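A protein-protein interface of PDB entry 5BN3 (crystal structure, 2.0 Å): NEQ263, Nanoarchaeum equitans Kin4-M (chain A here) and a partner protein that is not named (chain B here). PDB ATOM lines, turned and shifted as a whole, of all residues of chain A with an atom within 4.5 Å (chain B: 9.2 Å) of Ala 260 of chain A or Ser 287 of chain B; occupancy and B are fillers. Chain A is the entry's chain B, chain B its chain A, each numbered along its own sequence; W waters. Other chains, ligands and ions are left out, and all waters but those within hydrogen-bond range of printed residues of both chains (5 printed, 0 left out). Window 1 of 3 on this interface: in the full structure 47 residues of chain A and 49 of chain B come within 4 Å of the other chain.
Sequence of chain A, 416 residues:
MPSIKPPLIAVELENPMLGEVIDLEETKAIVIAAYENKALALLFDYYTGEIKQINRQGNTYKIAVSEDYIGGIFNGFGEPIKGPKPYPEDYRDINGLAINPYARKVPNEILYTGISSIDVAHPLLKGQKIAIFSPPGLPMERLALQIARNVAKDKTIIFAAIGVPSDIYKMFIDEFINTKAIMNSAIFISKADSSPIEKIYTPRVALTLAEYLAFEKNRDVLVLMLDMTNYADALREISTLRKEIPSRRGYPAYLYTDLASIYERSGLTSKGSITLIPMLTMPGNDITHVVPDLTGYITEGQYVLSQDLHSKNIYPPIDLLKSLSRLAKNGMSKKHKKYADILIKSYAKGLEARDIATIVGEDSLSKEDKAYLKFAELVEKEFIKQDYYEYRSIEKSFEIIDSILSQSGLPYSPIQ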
ATOM      1  N   TYR A 256      23.795  -0.809 -11.860  1.00  0.00           N
ATOM      2  CA  TYR A 256      24.831  -1.113 -12.844  1.00  0.00           C
ATOM      3  C   TYR A 256      24.217  -1.401 -14.208  1.00  0.00           C
ATOM      4  O   TYR A 256      24.656  -0.867 -15.227  1.00  0.00           O
ATOM      5  CB  TYR A 256      25.666  -2.314 -12.386  1.00  0.00           C
ATOM      6  CG  TYR A 256      26.659  -2.818 -13.414  1.00  0.00           C
ATOM      7  CD1 TYR A 256      26.300  -3.792 -14.340  1.00  0.00           C
ATOM      8  CD2 TYR A 256      27.958  -2.336 -13.448  1.00  0.00           C
ATOM      9  CE1 TYR A 256      27.201  -4.256 -15.276  1.00  0.00           C
ATOM     10  CE2 TYR A 256      28.870  -2.800 -14.380  1.00  0.00           C
ATOM     11  CZ  TYR A 256      28.484  -3.757 -15.291  1.00  0.00           C
ATOM     12  OH  TYR A 256      29.381  -4.225 -16.222  1.00  0.00           O
ATOM     13  N   THR A 257      23.205  -2.261 -14.223  1.00  0.00           N
ATOM     14  CA  THR A 257      22.569  -2.669 -15.470  1.00  0.00           C
ATOM     15  C   THR A 257      21.867  -1.494 -16.155  1.00  0.00           C
ATOM     16  O   THR A 257      21.914  -1.364 -17.375  1.00  0.00           O
ATOM     17  CB  THR A 257      21.585  -3.833 -15.235  1.00  0.00           C
ATOM     18  OG1 THR A 257      22.298  -4.944 -14.675  1.00  0.00           O
ATOM     19  CG2 THR A 257      20.939  -4.269 -16.537  1.00  0.00           C
ATOM     20  N   ASP A 258      21.232  -0.632 -15.368  1.00  0.00           N
ATOM     21  CA  ASP A 258      20.553   0.525 -15.935  1.00  0.00           C
ATOM     22  C   ASP A 258      21.541   1.541 -16.503  1.00  0.00           C
ATOM     23  O   ASP A 258      21.325   2.083 -17.587  1.00  0.00           O
ATOM     24  CB  ASP A 258      19.647   1.184 -14.898  1.00  0.00           C
ATOM     25  CG  ASP A 258      18.852   2.331 -15.475  1.00  0.00           C
ATOM     26  OD1 ASP A 258      17.736   2.091 -15.982  1.00  0.00           O
ATOM     27  OD2 ASP A 258      19.344   3.475 -15.434  1.00  0.00           O
ATOM     28  N   LEU A 259      22.625   1.799 -15.776  1.00  0.00           N
ATOM     29  CA  LEU A 259      23.672   2.693 -16.269  1.00  0.00           C
ATOM     30  C   LEU A 259      24.283   2.149 -17.558  1.00  0.00           C
ATOM     31  O   LEU A 259      24.571   2.901 -18.490  1.00  0.00           O
ATOM     32  CB  LEU A 259      24.756   2.896 -15.205  1.00  0.00           C
ATOM     33  CG  LEU A 259      24.395   3.764 -13.995  1.00  0.00           C
ATOM     34  CD1 LEU A 259      25.541   3.804 -12.988  1.00  0.00           C
ATOM     35  CD2 LEU A 259      24.034   5.173 -14.438  1.00  0.00           C
ATOM     36  N   ALA A 260      24.467   0.835 -17.608  1.00  0.00           N
ATOM     37  CA  ALA A 260      25.019   0.187 -18.791  1.00  0.00           C
ATOM     38  C   ALA A 260      24.076   0.302 -19.980  1.00  0.00           C
ATOM     39  O   ALA A 260      24.521   0.448 -21.116  1.00  0.00           O
ATOM     40  CB  ALA A 260      25.319  -1.262 -18.499  1.00  0.00           C
ATOM     41  N   SER A 261      22.773   0.241 -19.717  1.00  0.00           N
ATOM     42  CA  SER A 261      21.774   0.340 -20.781  1.00  0.00           C
ATOM     43  C   SER A 261      21.811   1.716 -21.442  1.00  0.00           C
ATOM     44  O   SER A 261      21.195   1.934 -22.483  1.00  0.00           O
ATOM     45  CB  SER A 261      20.374   0.052 -20.240  1.00  0.00           C
ATOM     46  OG  SER A 261      19.850   1.178 -19.561  1.00  0.00           O
ATOM     47  N   ILE A 262      22.541   2.640 -20.823  1.00  0.00           N
ATOM     48  CA  ILE A 262      22.782   3.957 -21.396  1.00  0.00           C
ATOM     49  C   ILE A 262      24.181   4.046 -22.013  1.00  0.00           C
ATOM     50  O   ILE A 262      24.324   4.390 -23.187  1.00  0.00           O
ATOM     51  CB  ILE A 262      22.610   5.047 -20.325  1.00  0.00           C
ATOM     52  CG1 ILE A 262      21.140   5.149 -19.920  1.00  0.00           C
ATOM     53  CG2 ILE A 262      23.097   6.391 -20.826  1.00  0.00           C
ATOM     54  CD1 ILE A 262      20.890   6.214 -18.913  1.00  0.00           C
ATOM     55  N   TYR A 263      25.207   3.734 -21.222  1.00  0.00           N
ATOM     56  CA  TYR A 263      26.598   3.873 -21.661  1.00  0.00           C
ATOM     57  C   TYR A 263      26.945   3.008 -22.876  1.00  0.00           C
ATOM     58  O   TYR A 263      27.736   3.417 -23.727  1.00  0.00           O
ATOM     59  CB  TYR A 263      27.558   3.544 -20.512  1.00  0.00           C
ATOM     60  CG  TYR A 263      27.450   4.442 -19.297  1.00  0.00           C
ATOM     61  CD1 TYR A 263      27.002   5.751 -19.404  1.00  0.00           C
ATOM     62  CD2 TYR A 263      27.809   3.975 -18.041  1.00  0.00           C
ATOM     63  CE1 TYR A 263      26.913   6.567 -18.286  1.00  0.00           C
ATOM     64  CE2 TYR A 263      27.722   4.782 -16.923  1.00  0.00           C
ATOM     65  CZ  TYR A 263      27.276   6.073 -17.052  1.00  0.00           C
ATOM     66  OH  TYR A 263      27.193   6.871 -15.934  1.00  0.00           O
ATOM     67  N   GLU A 264      26.362   1.815 -22.951  1.00  0.00           N
ATOM     68  CA  GLU A 264      26.677   0.876 -24.031  1.00  0.00           C
ATOM     69  C   GLU A 264      25.977   1.207 -25.347  1.00  0.00           C
ATOM     70  O   GLU A 264      26.208   0.547 -26.363  1.00  0.00           O
ATOM     71  CB  GLU A 264      26.365  -0.565 -23.607  1.00  0.00           C
ATOM     72  CG  GLU A 264      27.336  -1.126 -22.575  1.00  0.00           C
ATOM     73  CD  GLU A 264      28.654  -1.581 -23.184  1.00  0.00           C
ATOM     74  OE1 GLU A 264      29.713  -1.320 -22.574  1.00  0.00           O
ATOM     75  OE2 GLU A 264      28.636  -2.218 -24.259  1.00  0.00           O
ATOM     76  N   ILE A 298      32.050   0.415 -16.198  1.00  0.00           N
ATOM     77  CA  ILE A 298      31.352   0.361 -17.485  1.00  0.00           C
ATOM     78  C   ILE A 298      32.042   1.149 -18.601  1.00  0.00           C
ATOM     79  O   ILE A 298      32.301   0.606 -19.675  1.00  0.00           O
ATOM     80  CB  ILE A 298      29.898   0.856 -17.361  1.00  0.00           C
ATOM     81  CG1 ILE A 298      29.140  -0.002 -16.349  1.00  0.00           C
ATOM     82  CG2 ILE A 298      29.201   0.796 -18.713  1.00  0.00           C
ATOM     83  CD1 ILE A 298      27.894   0.664 -15.802  1.00  0.00           C
ATOM     84  N   GLY B 249      31.870 -13.788 -21.486  1.00  0.00           N
ATOM     85  CA  GLY B 249      31.675 -12.383 -21.188  1.00  0.00           C
ATOM     86  C   GLY B 249      30.360 -12.209 -20.458  1.00  0.00           C
ATOM     87  O   GLY B 249      29.307 -12.065 -21.083  1.00  0.00           O
ATOM     88  N   CYS B 250      30.423 -12.232 -19.131  1.00  0.00           N
ATOM     89  CA  CYS B 250      29.229 -12.151 -18.302  1.00  0.00           C
ATOM     90  C   CYS B 250      29.004 -10.723 -17.815  1.00  0.00           C
ATOM     91  O   CYS B 250      29.625 -10.287 -16.847  1.00  0.00           O
ATOM     92  CB  CYS B 250      29.351 -13.110 -17.115  1.00  0.00           C
ATOM     93  SG  CYS B 250      27.918 -13.158 -16.012  1.00  0.00           S
ATOM     94  N   GLY B 251      28.121  -9.999 -18.501  1.00  0.00           N
ATOM     95  CA  GLY B 251      27.731  -8.662 -18.092  1.00  0.00           C
ATOM     96  C   GLY B 251      28.798  -7.593 -18.242  1.00  0.00           C
ATOM     97  O   GLY B 251      28.790  -6.611 -17.499  1.00  0.00           O
ATOM     98  N   GLU B 252      29.707  -7.771 -19.200  1.00  0.00           N
ATOM     99  CA  GLU B 252      30.766  -6.786 -19.442  1.00  0.00           C
ATOM    100  C   GLU B 252      30.602  -6.053 -20.774  1.00  0.00           C
ATOM    101  O   GLU B 252      29.515  -6.052 -21.353  1.00  0.00           O
ATOM    102  CB  GLU B 252      32.148  -7.439 -19.352  1.00  0.00           C
ATOM    103  CG  GLU B 252      32.510  -7.924 -17.957  1.00  0.00           C
ATOM    104  CD  GLU B 252      32.619  -6.793 -16.951  1.00  0.00           C
ATOM    105  OE1 GLU B 252      33.180  -5.732 -17.300  1.00  0.00           O
ATOM    106  OE2 GLU B 252      32.144  -6.960 -15.807  1.00  0.00           O
ATOM    107  N   ARG B 253      31.678  -5.429 -21.252  1.00  0.00           N
ATOM    108  CA  ARG B 253      31.610  -4.558 -22.431  1.00  0.00           C
ATOM    109  C   ARG B 253      31.497  -5.317 -23.753  1.00  0.00           C
ATOM    110  O   ARG B 253      32.164  -6.335 -23.957  1.00  0.00           O
ATOM    111  CB  ARG B 253      32.821  -3.615 -22.483  1.00  0.00           C
ATOM    112  CG  ARG B 253      32.942  -2.694 -21.272  1.00  0.00           C
ATOM    113  CD  ARG B 253      34.166  -1.787 -21.357  1.00  0.00           C
ATOM    114  NE  ARG B 253      34.350  -1.024 -20.122  1.00  0.00           N
ATOM    115  CZ  ARG B 253      35.066  -1.443 -19.083  1.00  0.00           C
ATOM    116  NH1 ARG B 253      35.681  -2.615 -19.130  1.00  0.00           N
ATOM    117  NH2 ARG B 253      35.173  -0.691 -17.999  1.00  0.00           N
ATOM    118  N   GLY B 254      30.655  -4.807 -24.649  1.00  0.00           N
ATOM    119  CA  GLY B 254      30.495  -5.393 -25.967  1.00  0.00           C
ATOM    120  C   GLY B 254      31.780  -5.339 -26.770  1.00  0.00           C
ATOM    121  O   GLY B 254      32.118  -6.288 -27.479  1.00  0.00           O
ATOM    122  N   ASN B 255      32.501  -4.227 -26.652  1.00  0.00           N
ATOM    123  CA  ASN B 255      33.761  -4.044 -27.369  1.00  0.00           C
ATOM    124  C   ASN B 255      34.826  -5.081 -27.017  1.00  0.00           C
ATOM    125  O   ASN B 255      35.703  -5.372 -27.829  1.00  0.00           O
ATOM    126  CB  ASN B 255      34.313  -2.636 -27.132  1.00  0.00           C
ATOM    127  CG  ASN B 255      33.726  -1.610 -28.081  1.00  0.00           C
ATOM    128  OD1 ASN B 255      33.336  -1.936 -29.205  1.00  0.00           O
ATOM    129  ND2 ASN B 255      33.665  -0.359 -27.635  1.00  0.00           N
ATOM    130  N   GLU B 256      34.756  -5.627 -25.806  1.00  0.00           N
ATOM    131  CA  GLU B 256      35.746  -6.601 -25.359  1.00  0.00           C
ATOM    132  C   GLU B 256      35.532  -7.962 -26.016  1.00  0.00           C
ATOM    133  O   GLU B 256      36.486  -8.703 -26.252  1.00  0.00           O
ATOM    134  CB  GLU B 256      35.746  -6.704 -23.830  1.00  0.00           C
ATOM    135  CG  GLU B 256      36.336  -5.466 -23.158  1.00  0.00           C
ATOM    136  CD  GLU B 256      35.872  -5.279 -21.731  1.00  0.00           C
ATOM    137  OE1 GLU B 256      35.046  -6.087 -21.251  1.00  0.00           O
ATOM    138  OE2 GLU B 256      36.335  -4.314 -21.083  1.00  0.00           O
ATOM    139  N   MET B 257      34.279  -8.282 -26.317  1.00  0.00           N
ATOM    140  CA  MET B 257      33.973  -9.475 -27.097  1.00  0.00           C
ATOM    141  C   MET B 257      34.408  -9.269 -28.546  1.00  0.00           C
ATOM    142  O   MET B 257      34.993 -10.162 -29.163  1.00  0.00           O
ATOM    143  CB  MET B 257      32.474  -9.783 -27.029  1.00  0.00           C
ATOM    144  CG  MET B 257      31.916  -9.940 -25.620  1.00  0.00           C
ATOM    145  SD  MET B 257      32.346 -11.507 -24.831  1.00  0.00           S
ATOM    146  CE  MET B 257      33.899 -11.091 -24.038  1.00  0.00           C
ATOM    147  N   ALA B 284      28.762 -14.466 -25.065  1.00  0.00           N
ATOM    148  CA  ALA B 284      28.637 -13.044 -24.763  1.00  0.00           C
ATOM    149  C   ALA B 284      27.240 -12.655 -24.308  1.00  0.00           C
ATOM    150  O   ALA B 284      26.287 -12.727 -25.083  1.00  0.00           O
ATOM    151  CB  ALA B 284      29.033 -12.213 -25.972  1.00  0.00           C
ATOM    152  N   ASN B 285      27.127 -12.237 -23.053  1.00  0.00           N
ATOM    153  CA  ASN B 285      25.931 -11.551 -22.589  1.00  0.00           C
ATOM    154  C   ASN B 285      26.362 -10.238 -21.953  1.00  0.00           C
ATOM    155  O   ASN B 285      26.654 -10.180 -20.758  1.00  0.00           O
ATOM    156  CB  ASN B 285      25.138 -12.403 -21.600  1.00  0.00           C
ATOM    157  CG  ASN B 285      23.686 -11.974 -21.501  1.00  0.00           C
ATOM    158  OD1 ASN B 285      22.868 -12.319 -22.354  1.00  0.00           O
ATOM    159  ND2 ASN B 285      23.359 -11.218 -20.458  1.00  0.00           N
ATOM    160  N   THR B 286      26.411  -9.191 -22.771  1.00  0.00           N
ATOM    161  CA  THR B 286      26.959  -7.902 -22.363  1.00  0.00           C
ATOM    162  C   THR B 286      26.141  -7.230 -21.268  1.00  0.00           C
ATOM    163  O   THR B 286      25.027  -7.654 -20.961  1.00  0.00           O
ATOM    164  CB  THR B 286      27.106  -6.950 -23.563  1.00  0.00           C
ATOM    165  OG1 THR B 286      25.814  -6.676 -24.119  1.00  0.00           O
ATOM    166  CG2 THR B 286      27.984  -7.579 -24.626  1.00  0.00           C
ATOM    167  N   SER B 287      26.709  -6.176 -20.689  1.00  0.00           N
ATOM    168  CA  SER B 287      26.109  -5.480 -19.558  1.00  0.00           C
ATOM    169  C   SER B 287      24.675  -5.017 -19.809  1.00  0.00           C
ATOM    170  O   SER B 287      23.847  -5.031 -18.892  1.00  0.00           O
ATOM    171  CB  SER B 287      26.983  -4.290 -19.167  1.00  0.00           C
ATOM    172  OG  SER B 287      27.158  -3.419 -20.266  1.00  0.00           O
ATOM    173  N   ASN B 288      24.378  -4.613 -21.042  1.00  0.00           N
ATOM    174  CA  ASN B 288      23.036  -4.126 -21.374  1.00  0.00           C
ATOM    175  C   ASN B 288      22.123  -5.156 -22.053  1.00  0.00           C
ATOM    176  O   ASN B 288      21.015  -4.826 -22.480  1.00  0.00           O
ATOM    177  CB  ASN B 288      23.105  -2.837 -22.202  1.00  0.00           C
ATOM    178  CG  ASN B 288      23.704  -3.053 -23.578  1.00  0.00           C
ATOM    179  OD1 ASN B 288      24.534  -3.940 -23.780  1.00  0.00           O
ATOM    180  ND2 ASN B 288      23.290  -2.229 -24.534  1.00  0.00           N
ATOM    181  N   MET B 289      22.591  -6.397 -22.158  1.00  0.00           N
ATOM    182  CA  MET B 289      21.745  -7.500 -22.616  1.00  0.00           C
ATOM    183  C   MET B 289      20.937  -7.977 -21.401  1.00  0.00           C
ATOM    184  O   MET B 289      21.249  -7.571 -20.279  1.00  0.00           O
ATOM    185  CB  MET B 289      22.610  -8.603 -23.254  1.00  0.00           C
ATOM    186  CG  MET B 289      22.985  -8.298 -24.711  1.00  0.00           C
ATOM    187  SD  MET B 289      24.346  -9.266 -25.405  1.00  0.00           S
ATOM    188  CE  MET B 289      23.534 -10.829 -25.742  1.00  0.00           C
ATOM    189  N   PRO B 290      19.879  -8.794 -21.610  1.00  0.00           N
ATOM    190  CA  PRO B 290      19.004  -9.135 -20.476  1.00  0.00           C
ATOM    191  C   PRO B 290      19.752  -9.688 -19.257  1.00  0.00           C
ATOM    192  O   PRO B 290      20.600 -10.572 -19.399  1.00  0.00           O
ATOM    193  CB  PRO B 290      18.076 -10.205 -21.060  1.00  0.00           C
ATOM    194  CG  PRO B 290      18.019  -9.882 -22.515  1.00  0.00           C
ATOM    195  CD  PRO B 290      19.398  -9.400 -22.867  1.00  0.00           C
ATOM    196  N   ILE B 291      19.430  -9.164 -18.077  1.00  0.00           N
ATOM    197  CA  ILE B 291      20.176  -9.473 -16.857  1.00  0.00           C
ATOM    198  C   ILE B 291      20.122 -10.952 -16.463  1.00  0.00           C
ATOM    199  O   ILE B 291      21.127 -11.517 -16.032  1.00  0.00           O
ATOM    200  CB  ILE B 291      19.746  -8.547 -15.671  1.00  0.00           C
ATOM    201  CG1 ILE B 291      20.729  -8.660 -14.502  1.00  0.00           C
ATOM    202  CG2 ILE B 291      18.312  -8.836 -15.216  1.00  0.00           C
ATOM    203  CD1 ILE B 291      20.522  -7.614 -13.427  1.00  0.00           C
ATOM    204  N   ALA B 292      18.964 -11.582 -16.635  1.00  0.00           N
ATOM    205  CA  ALA B 292      18.797 -12.984 -16.256  1.00  0.00           C
ATOM    206  C   ALA B 292      19.621 -13.925 -17.133  1.00  0.00           C
ATOM    207  O   ALA B 292      19.949 -15.041 -16.725  1.00  0.00           O
ATOM    208  CB  ALA B 292      17.330 -13.367 -16.295  1.00  0.00           C
ATOM    209  N   ARG B 294      22.602 -13.560 -17.853  1.00  0.00           N
ATOM    210  CA  ARG B 294      23.936 -13.664 -17.263  1.00  0.00           C
ATOM    211  C   ARG B 294      24.087 -14.985 -16.528  1.00  0.00           C
ATOM    212  O   ARG B 294      25.129 -15.634 -16.608  1.00  0.00           O
ATOM    213  CB  ARG B 294      24.192 -12.519 -16.279  1.00  0.00           C
ATOM    214  CG  ARG B 294      24.276 -11.144 -16.904  1.00  0.00           C
ATOM    215  CD  ARG B 294      24.583 -10.097 -15.851  1.00  0.00           C
ATOM    216  NE  ARG B 294      24.363  -8.744 -16.355  1.00  0.00           N
ATOM    217  CZ  ARG B 294      24.389  -7.653 -15.601  1.00  0.00           C
ATOM    218  NH1 ARG B 294      24.629  -7.752 -14.300  1.00  0.00           N
ATOM    219  NH2 ARG B 294      24.174  -6.468 -16.146  1.00  0.00           N
ATOM    220  N   ASP B 320      34.147 -13.593 -16.948  1.00  0.00           N
ATOM    221  CA  ASP B 320      34.382 -12.171 -16.716  1.00  0.00           C
ATOM    222  C   ASP B 320      33.077 -11.410 -16.952  1.00  0.00           C
ATOM    223  O   ASP B 320      32.701 -11.182 -18.098  1.00  0.00           O
ATOM    224  CB  ASP B 320      35.464 -11.686 -17.695  1.00  0.00           C
ATOM    225  CG  ASP B 320      35.794 -10.211 -17.541  1.00  0.00           C
ATOM    226  OD1 ASP B 320      35.550  -9.640 -16.458  1.00  0.00           O
ATOM    227  OD2 ASP B 320      36.320  -9.617 -18.511  1.00  0.00           O
ATOM    228  N   SER B 321      32.376 -11.014 -15.890  1.00  0.00           N
ATOM    229  CA  SER B 321      32.802 -11.194 -14.506  1.00  0.00           C
ATOM    230  C   SER B 321      31.696 -11.844 -13.674  1.00  0.00           C
ATOM    231  O   SER B 321      30.510 -11.623 -13.927  1.00  0.00           O
ATOM    232  CB  SER B 321      33.172  -9.833 -13.907  1.00  0.00           C
ATOM    233  OG  SER B 321      32.991  -9.823 -12.504  1.00  0.00           O
ATOM    234  N   ARG B 324      28.698  -9.876 -11.965  1.00  0.00           N
ATOM    235  CA  ARG B 324      27.523  -9.485 -12.743  1.00  0.00           C
ATOM    236  C   ARG B 324      26.432 -10.545 -12.628  1.00  0.00           C
ATOM    237  O   ARG B 324      25.242 -10.232 -12.643  1.00  0.00           O
ATOM    238  CB  ARG B 324      27.899  -9.265 -14.212  1.00  0.00           C
ATOM    239  CG  ARG B 324      29.090  -8.336 -14.420  1.00  0.00           C
ATOM    240  CD  ARG B 324      28.913  -7.026 -13.678  1.00  0.00           C
ATOM    241  NE  ARG B 324      30.124  -6.215 -13.739  1.00  0.00           N
ATOM    242  CZ  ARG B 324      30.516  -5.382 -12.781  1.00  0.00           C
ATOM    243  NH1 ARG B 324      29.792  -5.246 -11.679  1.00  0.00           N
ATOM    244  NH2 ARG B 324      31.636  -4.688 -12.927  1.00  0.00           N
ATOM    245  N   GLU B 327      24.876  -9.973  -9.349  1.00  0.00           N
ATOM    246  CA  GLU B 327      23.909  -8.878  -9.445  1.00  0.00           C
ATOM    247  C   GLU B 327      22.571  -9.377  -9.982  1.00  0.00           C
ATOM    248  O   GLU B 327      21.511  -8.930  -9.545  1.00  0.00           O
ATOM    249  CB  GLU B 327      24.432  -7.760 -10.350  1.00  0.00           C
ATOM    250  CG  GLU B 327      23.432  -6.619 -10.540  1.00  0.00           C
ATOM    251  CD  GLU B 327      23.790  -5.686 -11.682  1.00  0.00           C
ATOM    252  OE1 GLU B 327      24.866  -5.868 -12.289  1.00  0.00           O
ATOM    253  OE2 GLU B 327      22.992  -4.765 -11.977  1.00  0.00           O
HETATM  254  O   HOH W   1      29.566  -2.449 -20.101  1.00  0.00           O
HETATM  255  O   HOH W   2      31.132  -1.755 -25.767  1.00  0.00           O
HETATM  256  O   HOH W   3      24.277  -1.275 -27.117  1.00  0.00           O
HETATM  257  O   HOH W   4      26.959  -3.573 -25.484  1.00  0.00           O
HETATM  258  O   HOH W   5      31.406  -3.359 -18.219  1.00  0.00           O
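Hydrophobic or aromatic side chains of chain A within 4 Å of the printed part of chain B: Tyr 256 and Ala 260. Of the 23 printed residues of chain B, 10 touch a printed residue of chain A. Hydrophobic or aromatic side chains of chain B that line the printed part of chain A: Ile 291.
Among the printed residues, merely in contact across the chains: Tyr 256 of chain A with Glu 327 of chain B (3.3 Å), Glu 264 of chain A with Ser 287 of chain B (3.3 Å), Ala 260 of chain A with Ser 287 of chain B (3.3 Å), Thr 257 of chain A with Ile 291 of chain B (3.4 Å), Glu 264 of chain A with Asn 288 of chain B (3.6 Å), Ser 261 of chain A with Asn 288 of chain B (3.7 Å), Ala 260 of chain A with Asn 288 of chain B (3.7 Å), Glu 264 of chain A with Arg 253 of chain B (3.7 Å), Tyr 256 of chain A with Ser 287 of chain B (3.8 Å), Thr 257 of chain A with Ser 287 of chain B (3.8 Å), Tyr 256 of chain A with Arg 294 of chain B (3.8 Å) and Tyr 256 of chain A with Glu 252 of chain B (3.9 Å).
NH2 of Arg 294 of chain B is in hydrogen-bond range of OG1 of Thr 257 of chain A (2.8 Å). The side-chain carboxylate (OE2) of Glu 327 of chain B lies within hydrogen-bond range of the side-chain hydroxyl (OG1) of Thr 257 of chain A (2.8 Å). The side-chain carboxylate of Glu 264 of chain A sits at hydrogen-bond distance from the backbone NH of Gly 254 of chain B, 3.3 Å away. The backbone carbonyl oxygen (O) of Gly 251 of chain B sits at hydrogen-bond distance from the side-chain hydroxyl (OH) of Tyr 256 of chain A, 2.8 Å away. The guanidinium group (NE) of Arg 324 of chain B lies within hydrogen-bond range of the side-chain hydroxyl (OH) of Tyr 256 of chain A (3.3 Å). NE of Arg 253 of chain B sits at hydrogen-bond distance from O of Ile 298 of chain A (2.7 Å).
Of chain B, only Ser 287 and Asn 288 come within 4 Å of Ala 260 of chain A. Ser 287 of chain B touches four residues of chain A. Thr 257 of chain A touches just these residues of chain B: Ser 287 (3.8 Å), Ile 291 (3.4 Å), Arg 294 (2.8 Å) and Glu 327 (2.8 Å). Printed residues of chain A within 4 Å of Glu 327 of chain B: Tyr 256 and Thr 257. Of the printed residues of chain A, Glu 252 of chain B touches Tyr 256. Of the printed residues of chain B, Ile 298 of chain A touches Arg 253 (2.7 Å). Of the printed residues of chain A, Gly 254 of chain B touches Glu 264. Glu 256 of chain B touches none of the printed residues of chain A. Pro 290 of chain B touches none of the printed residues of chain A. The nearest printed residue of chain A that does not touch Ser 287 of chain B is Ile 298 of chain A (4.9 Å). The nearest printed residue of chain A that does not touch Arg 253 of chain B is Tyr 256 of chain A (5.7 Å).
Water W4 bridges OE2 of Glu 264 of chain A (2.5 Å) and OD1 of Asn 288 of chain B (3.0 Å). Water W1 lies within hydrogen-bond range of OG of Ser 287 of chain B (2.6 Å) and OE1 of Glu 264 of chain A (2.7 Å). Water W3 bridges the backbone carbonyl oxygen of Glu 264 of chain A (2.8 Å) and the side-chain amide nitrogen of Asn 288 of chain B (2.9 Å). Water W2 lies within hydrogen-bond range of the side-chain carboxylate (OE2) of Glu 264 of chain A, the backbone NH (N) of Asn 255 of chain B and the backbone NH (N) of Gly 254 of chain B. Water W5 bridges OH of Tyr 256 of chain A and OE1 of Glu 252 of chain B.
The backbone carbonyl oxygen (O) of Glu 252 of chain B sits at hydrogen-bond distance from the backbone NH (N) of Ser 287 of chain B (2.9 Å). The backbone NH (N) of Gly 251 of chain B sits at hydrogen-bond distance from the backbone carbonyl oxygen (O) of Asn 285 of chain B (2.7 Å). The backbone carbonyl oxygen (O) of Arg 324 of chain B is in hydrogen-bond range of the guanidinium group (NH1) of Arg 294 of chain B (3.0 Å). SG of Cys 250 of chain B sits at hydrogen-bond distance from O of Arg 294 of chain B (3.8 Å). The guanidinium group of Arg 253 of chain B lies within salt-bridge range of the side-chain carboxylate of Glu 256 of chain B (2.7 Å). The side-chain carboxylate of Glu 252 of chain B is in salt-bridge range of the guanidinium group of Arg 324 of chain B (3.0 Å).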
